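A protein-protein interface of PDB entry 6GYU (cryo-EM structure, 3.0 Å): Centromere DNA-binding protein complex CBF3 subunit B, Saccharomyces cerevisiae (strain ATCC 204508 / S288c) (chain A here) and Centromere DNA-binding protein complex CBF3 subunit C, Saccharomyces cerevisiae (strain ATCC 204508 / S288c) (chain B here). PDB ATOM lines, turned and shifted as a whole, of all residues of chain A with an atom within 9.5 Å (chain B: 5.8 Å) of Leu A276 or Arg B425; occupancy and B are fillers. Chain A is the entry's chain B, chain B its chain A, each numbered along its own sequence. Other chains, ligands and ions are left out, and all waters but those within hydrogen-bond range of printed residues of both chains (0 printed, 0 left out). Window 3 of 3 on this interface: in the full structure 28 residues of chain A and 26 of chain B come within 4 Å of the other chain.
Among the printed residues, merely in contact across the chains: Pro A274 with Leu B424 (3.8 Å), Pro A274 with Ala B428 (3.3 Å), Pro A280 with Ile B421 (3.8 Å) and Val A287 with Leu B424 (3.9 Å).
NE of Arg B425 is in salt-bridge range of OE2 of Glu B379, 2.4 Å away.
Of chain B, only Arg B425 comes within 4 Å of Leu A276.
Of the printed residues of chain A, Leu B424 touches Pro A274 (3.8 Å) and Val A287 (3.9 Å).
Printed residues of chain B within 4 Å of Val A287: Leu B424 (3.9 Å).
Gln B427 touches none of the printed residues of chain A.
The nearest residue of chain B that does not touch Leu A276 is Ala B428 (4.4 Å).
The nearest printed residue of chain A that does not touch Arg B425 is Asn A277 (4.6 Å).
The nearest printed residue of chain B that does not touch Val A287 is Gln B427 (7.6 Å).
O of Leu A276 sits at hydrogen-bond distance from NH1 of Arg B425 (2.4 Å).
Hydrophobic or aromatic side chains of chain A that line the printed part of chain B: Pro A274, Pro A280 and Val A287.
Of the 11 printed residues of chain B, 4 touch a printed residue of chain A.
Hydrophobic or aromatic side chains of chain B within 4 Å of the printed part of chain A: Ile B421, Leu B424 and Ala B428.
Among the printed residues, 5 pairs touch across the chains.
Among the printed residues, no Asp or Glu carboxylate lies within 4 Å of a Lys or Arg side-chain nitrogen of the other chain.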
ATOM      1  N   ARG A 273      18.065  -3.735  24.207  1.00  0.00           N
ATOM      2  CA  ARG A 273      18.169  -4.211  22.839  1.00  0.00           C
ATOM      3  C   ARG A 273      17.499  -5.575  22.738  1.00  0.00           C
ATOM      4  O   ARG A 273      17.823  -6.473  23.523  1.00  0.00           O
ATOM      5  CB  ARG A 273      19.633  -4.309  22.440  1.00  0.00           C
ATOM      6  CG  ARG A 273      20.344  -2.978  22.375  1.00  0.00           C
ATOM      7  CD  ARG A 273      21.836  -3.173  22.203  1.00  0.00           C
ATOM      8  NE  ARG A 273      22.434  -3.734  23.409  1.00  0.00           N
ATOM      9  CZ  ARG A 273      23.701  -4.113  23.516  1.00  0.00           C
ATOM     10  NH1 ARG A 273      24.518  -3.987  22.487  1.00  0.00           N
ATOM     11  NH2 ARG A 273      24.150  -4.613  24.657  1.00  0.00           N
ATOM     12  N   PRO A 274      16.543  -5.755  21.829  1.00  0.00           N
ATOM     13  CA  PRO A 274      15.882  -7.059  21.700  1.00  0.00           C
ATOM     14  C   PRO A 274      16.837  -8.101  21.141  1.00  0.00           C
ATOM     15  O   PRO A 274      17.480  -7.884  20.112  1.00  0.00           O
ATOM     16  CB  PRO A 274      14.734  -6.776  20.728  1.00  0.00           C
ATOM     17  CG  PRO A 274      14.511  -5.311  20.821  1.00  0.00           C
ATOM     18  CD  PRO A 274      15.868  -4.721  21.032  1.00  0.00           C
ATOM     19  N   LEU A 275      16.929  -9.232  21.829  1.00  0.00           N
ATOM     20  CA  LEU A 275      17.822 -10.307  21.426  1.00  0.00           C
ATOM     21  C   LEU A 275      17.206 -11.075  20.258  1.00  0.00           C
ATOM     22  O   LEU A 275      16.099 -10.784  19.797  1.00  0.00           O
ATOM     23  CB  LEU A 275      18.121 -11.215  22.614  1.00  0.00           C
ATOM     24  CG  LEU A 275      18.912 -10.583  23.756  1.00  0.00           C
ATOM     25  CD1 LEU A 275      19.008 -11.536  24.933  1.00  0.00           C
ATOM     26  CD2 LEU A 275      20.293 -10.186  23.275  1.00  0.00           C
ATOM     27  N   LEU A 276      17.924 -12.080  19.770  1.00  0.00           N
ATOM     28  CA  LEU A 276      17.463 -12.865  18.637  1.00  0.00           C
ATOM     29  C   LEU A 276      16.561 -14.021  19.053  1.00  0.00           C
ATOM     30  O   LEU A 276      15.775 -14.504  18.231  1.00  0.00           O
ATOM     31  CB  LEU A 276      18.677 -13.377  17.854  1.00  0.00           C
ATOM     32  N   ASN A 277      16.635 -14.454  20.308  1.00  0.00           N
ATOM     33  CA  ASN A 277      15.827 -15.561  20.815  1.00  0.00           C
ATOM     34  C   ASN A 277      14.616 -15.079  21.601  1.00  0.00           C
ATOM     35  O   ASN A 277      14.223 -15.699  22.592  1.00  0.00           O
ATOM     36  CB  ASN A 277      16.688 -16.501  21.657  1.00  0.00           C
ATOM     37  N   ASP A 278      14.010 -13.971  21.186  1.00  0.00           N
ATOM     38  CA  ASP A 278      12.912 -13.357  21.917  1.00  0.00           C
ATOM     39  C   ASP A 278      11.586 -13.563  21.201  1.00  0.00           C
ATOM     40  O   ASP A 278      11.538 -13.682  19.973  1.00  0.00           O
ATOM     41  CB  ASP A 278      13.149 -11.860  22.113  1.00  0.00           C
ATOM     42  CG  ASP A 278      14.232 -11.570  23.124  1.00  0.00           C
ATOM     43  OD1 ASP A 278      14.420 -12.388  24.045  1.00  0.00           O
ATOM     44  OD2 ASP A 278      14.890 -10.519  23.001  1.00  0.00           O
ATOM     45  N   ASP A 279      10.525 -13.634  21.996  1.00  0.00           N
ATOM     46  CA  ASP A 279       9.169 -13.466  21.498  1.00  0.00           C
ATOM     47  C   ASP A 279       9.057 -12.095  20.832  1.00  0.00           C
ATOM     48  O   ASP A 279       9.578 -11.110  21.366  1.00  0.00           O
ATOM     49  CB  ASP A 279       8.197 -13.582  22.681  1.00  0.00           C
ATOM     50  CG  ASP A 279       6.744 -13.777  22.270  1.00  0.00           C
ATOM     51  OD1 ASP A 279       6.431 -13.865  21.073  1.00  0.00           O
ATOM     52  OD2 ASP A 279       5.893 -13.842  23.182  1.00  0.00           O
ATOM     53  N   PRO A 280       8.440 -11.997  19.647  1.00  0.00           N
ATOM     54  CA  PRO A 280       8.203 -10.668  19.051  1.00  0.00           C
ATOM     55  C   PRO A 280       7.320  -9.739  19.877  1.00  0.00           C
ATOM     56  O   PRO A 280       7.357  -8.524  19.654  1.00  0.00           O
ATOM     57  CB  PRO A 280       7.554 -11.006  17.706  1.00  0.00           C
ATOM     58  CG  PRO A 280       8.149 -12.311  17.354  1.00  0.00           C
ATOM     59  CD  PRO A 280       8.314 -13.065  18.641  1.00  0.00           C
ATOM     60  N   GLU A 282       7.766  -9.810  23.255  1.00  0.00           N
ATOM     61  CA  GLU A 282       8.787  -9.476  24.244  1.00  0.00           C
ATOM     62  C   GLU A 282       9.769  -8.432  23.724  1.00  0.00           C
ATOM     63  O   GLU A 282      10.262  -7.608  24.500  1.00  0.00           O
ATOM     64  CB  GLU A 282       9.528 -10.749  24.661  1.00  0.00           C
ATOM     65  CG  GLU A 282      10.582 -10.577  25.737  1.00  0.00           C
ATOM     66  CD  GLU A 282      11.260 -11.883  26.097  1.00  0.00           C
ATOM     67  OE1 GLU A 282      10.904 -12.920  25.500  1.00  0.00           O
ATOM     68  OE2 GLU A 282      12.154 -11.871  26.971  1.00  0.00           O
ATOM     69  N   SER A 283      10.036  -8.429  22.415  1.00  0.00           N
ATOM     70  CA  SER A 283      10.933  -7.435  21.833  1.00  0.00           C
ATOM     71  C   SER A 283      10.342  -6.032  21.910  1.00  0.00           C
ATOM     72  O   SER A 283      11.025  -5.085  22.320  1.00  0.00           O
ATOM     73  CB  SER A 283      11.242  -7.808  20.386  1.00  0.00           C
ATOM     74  OG  SER A 283      11.955  -9.029  20.322  1.00  0.00           O
ATOM     75  N   LYS A 286      10.406  -4.900  25.496  1.00  0.00           N
ATOM     76  CA  LYS A 286      11.694  -4.389  25.952  1.00  0.00           C
ATOM     77  C   LYS A 286      12.033  -3.045  25.323  1.00  0.00           C
ATOM     78  O   LYS A 286      12.721  -2.237  25.952  1.00  0.00           O
ATOM     79  CB  LYS A 286      12.805  -5.397  25.677  1.00  0.00           C
ATOM     80  CG  LYS A 286      12.735  -6.623  26.557  1.00  0.00           C
ATOM     81  CD  LYS A 286      14.009  -7.433  26.472  1.00  0.00           C
ATOM     82  CE  LYS A 286      14.112  -8.152  25.151  1.00  0.00           C
ATOM     83  NZ  LYS A 286      15.297  -9.049  25.111  1.00  0.00           N
ATOM     84  N   VAL A 287      11.549  -2.772  24.108  1.00  0.00           N
ATOM     85  CA  VAL A 287      11.723  -1.440  23.525  1.00  0.00           C
ATOM     86  C   VAL A 287      10.946  -0.392  24.323  1.00  0.00           C
ATOM     87  O   VAL A 287      11.472   0.689  24.645  1.00  0.00           O
ATOM     88  CB  VAL A 287      11.312  -1.454  22.040  1.00  0.00           C
ATOM     89  CG1 VAL A 287      11.259  -0.050  21.475  1.00  0.00           C
ATOM     90  CG2 VAL A 287      12.298  -2.270  21.239  1.00  0.00           C
ATOM     91  N   GLU B 379      19.163 -13.897   8.035  1.00  0.00           N
ATOM     92  CA  GLU B 379      18.037 -13.538   8.891  1.00  0.00           C
ATOM     93  C   GLU B 379      16.793 -13.208   8.074  1.00  0.00           C
ATOM     94  O   GLU B 379      15.760 -13.873   8.208  1.00  0.00           O
ATOM     95  CB  GLU B 379      18.410 -12.364   9.801  1.00  0.00           C
ATOM     96  CG  GLU B 379      17.277 -11.909  10.706  1.00  0.00           C
ATOM     97  CD  GLU B 379      16.890 -12.949  11.740  1.00  0.00           C
ATOM     98  OE1 GLU B 379      17.762 -13.740  12.162  1.00  0.00           O
ATOM     99  OE2 GLU B 379      15.704 -12.980  12.127  1.00  0.00           O
ATOM    100  N   ILE B 421       9.443  -5.995  13.237  1.00  0.00           N
ATOM    101  CA  ILE B 421      10.134  -7.196  13.648  1.00  0.00           C
ATOM    102  C   ILE B 421      11.003  -7.550  12.452  1.00  0.00           C
ATOM    103  O   ILE B 421      10.811  -7.017  11.359  1.00  0.00           O
ATOM    104  CB  ILE B 421       9.172  -8.341  14.052  1.00  0.00           C
ATOM    105  CG1 ILE B 421       9.877  -9.349  14.961  1.00  0.00           C
ATOM    106  CG2 ILE B 421       8.613  -9.041  12.826  1.00  0.00           C
ATOM    107  CD1 ILE B 421      10.296  -8.770  16.293  1.00  0.00           C
ATOM    108  N   THR B 422      12.053  -8.350  12.697  1.00  0.00           N
ATOM    109  CA  THR B 422      13.222  -8.669  11.856  1.00  0.00           C
ATOM    110  C   THR B 422      13.953  -7.421  11.337  1.00  0.00           C
ATOM    111  O   THR B 422      14.818  -7.510  10.459  1.00  0.00           O
ATOM    112  CB  THR B 422      12.885  -9.674  10.717  1.00  0.00           C
ATOM    113  OG1 THR B 422      14.102 -10.274  10.259  1.00  0.00           O
ATOM    114  CG2 THR B 422      12.199  -9.082   9.477  1.00  0.00           C
ATOM    115  N   TYR B 423      13.659  -6.266  11.935  1.00  0.00           N
ATOM    116  CA  TYR B 423      14.484  -5.071  11.973  1.00  0.00           C
ATOM    117  C   TYR B 423      15.262  -5.000  13.272  1.00  0.00           C
ATOM    118  O   TYR B 423      16.442  -4.637  13.275  1.00  0.00           O
ATOM    119  CB  TYR B 423      13.603  -3.823  11.850  1.00  0.00           C
ATOM    120  CG  TYR B 423      14.345  -2.512  11.803  1.00  0.00           C
ATOM    121  CD1 TYR B 423      14.926  -2.068  10.628  1.00  0.00           C
ATOM    122  CD2 TYR B 423      14.455  -1.712  12.934  1.00  0.00           C
ATOM    123  CE1 TYR B 423      15.594  -0.863  10.577  1.00  0.00           C
ATOM    124  CE2 TYR B 423      15.132  -0.511  12.894  1.00  0.00           C
ATOM    125  CZ  TYR B 423      15.704  -0.095  11.713  1.00  0.00           C
ATOM    126  OH  TYR B 423      16.377   1.103  11.662  1.00  0.00           O
ATOM    127  N   LEU B 424      14.602  -5.348  14.378  1.00  0.00           N
ATOM    128  CA  LEU B 424      15.279  -5.471  15.658  1.00  0.00           C
ATOM    129  C   LEU B 424      16.145  -6.720  15.702  1.00  0.00           C
ATOM    130  O   LEU B 424      17.146  -6.754  16.422  1.00  0.00           O
ATOM    131  CB  LEU B 424      14.250  -5.491  16.784  1.00  0.00           C
ATOM    132  CG  LEU B 424      13.398  -4.226  16.876  1.00  0.00           C
ATOM    133  CD1 LEU B 424      12.309  -4.385  17.918  1.00  0.00           C
ATOM    134  CD2 LEU B 424      14.263  -3.020  17.179  1.00  0.00           C
ATOM    135  N   ARG B 425      15.781  -7.751  14.939  1.00  0.00           N
ATOM    136  CA  ARG B 425      16.644  -8.919  14.802  1.00  0.00           C
ATOM    137  C   ARG B 425      17.822  -8.622  13.884  1.00  0.00           C
ATOM    138  O   ARG B 425      18.946  -9.070  14.141  1.00  0.00           O
ATOM    139  CB  ARG B 425      15.836 -10.101  14.275  1.00  0.00           C
ATOM    140  CG  ARG B 425      14.764 -10.573  15.233  1.00  0.00           C
ATOM    141  CD  ARG B 425      13.920 -11.660  14.612  1.00  0.00           C
ATOM    142  NE  ARG B 425      14.704 -12.854  14.321  1.00  0.00           N
ATOM    143  CZ  ARG B 425      14.907 -13.841  15.184  1.00  0.00           C
ATOM    144  NH1 ARG B 425      14.379 -13.779  16.399  1.00  0.00           N
ATOM    145  NH2 ARG B 425      15.632 -14.892  14.832  1.00  0.00           N
ATOM    146  N   CYS B 426      17.584  -7.845  12.826  1.00  0.00           N
ATOM    147  CA  CYS B 426      18.656  -7.404  11.944  1.00  0.00           C
ATOM    148  C   CYS B 426      19.609  -6.444  12.644  1.00  0.00           C
ATOM    149  O   CYS B 426      20.777  -6.351  12.257  1.00  0.00           O
ATOM    150  CB  CYS B 426      18.052  -6.755  10.698  1.00  0.00           C
ATOM    151  SG  CYS B 426      19.223  -6.298   9.413  1.00  0.00           S
ATOM    152  N   GLN B 427      19.140  -5.745  13.674  1.00  0.00           N
ATOM    153  CA  GLN B 427      19.986  -4.913  14.515  1.00  0.00           C
ATOM    154  C   GLN B 427      20.658  -5.721  15.620  1.00  0.00           C
ATOM    155  O   GLN B 427      21.787  -5.404  16.027  1.00  0.00           O
ATOM    156  CB  GLN B 427      19.139  -3.781  15.100  1.00  0.00           C
ATOM    157  CG  GLN B 427      19.887  -2.713  15.850  1.00  0.00           C
ATOM    158  CD  GLN B 427      18.974  -1.581  16.271  1.00  0.00           C
ATOM    159  OE1 GLN B 427      17.772  -1.612  16.010  1.00  0.00           O
ATOM    160  NE2 GLN B 427      19.540  -0.574  16.927  1.00  0.00           N
ATOM    161  N   ALA B 428      19.997  -6.781  16.088  1.00  0.00           N
ATOM    162  CA  ALA B 428      20.600  -7.693  17.047  1.00  0.00           C
ATOM    163  C   ALA B 428      21.735  -8.499  16.440  1.00  0.00           C
ATOM    164  O   ALA B 428      22.641  -8.895  17.171  1.00  0.00           O
ATOM    165  CB  ALA B 428      19.545  -8.637  17.615  1.00  0.00           C
ATOM    166  N   ILE B 429      21.701  -8.744  15.127  1.00  0.00           N
ATOM    167  CA  ILE B 429      22.853  -9.320  14.427  1.00  0.00           C
ATOM    168  C   ILE B 429      24.071  -8.409  14.554  1.00  0.00           C
ATOM    169  O   ILE B 429      25.183  -8.857  14.877  1.00  0.00           O
ATOM    170  CB  ILE B 429      22.503  -9.579  12.949  1.00  0.00           C
ATOM    171  CG1 ILE B 429      21.489 -10.710  12.817  1.00  0.00           C
ATOM    172  CG2 ILE B 429      23.744  -9.896  12.141  1.00  0.00           C
ATOM    173  CD1 ILE B 429      22.030 -12.038  13.254  1.00  0.00           C
ATOM    174  N   VAL B 430      23.865  -7.109  14.333  1.00  0.00           N
ATOM    175  CA  VAL B 430      24.960  -6.141  14.367  1.00  0.00           C
ATOM    176  C   VAL B 430      25.512  -6.011  15.782  1.00  0.00           C
ATOM    177  O   VAL B 430      26.732  -5.981  15.994  1.00  0.00           O
ATOM    178  CB  VAL B 430      24.478  -4.787  13.822  1.00  0.00           C
ATOM    179  CG1 VAL B 430      25.602  -3.785  13.823  1.00  0.00           C
ATOM    180  CG2 VAL B 430      23.902  -4.955  12.434  1.00  0.00           C
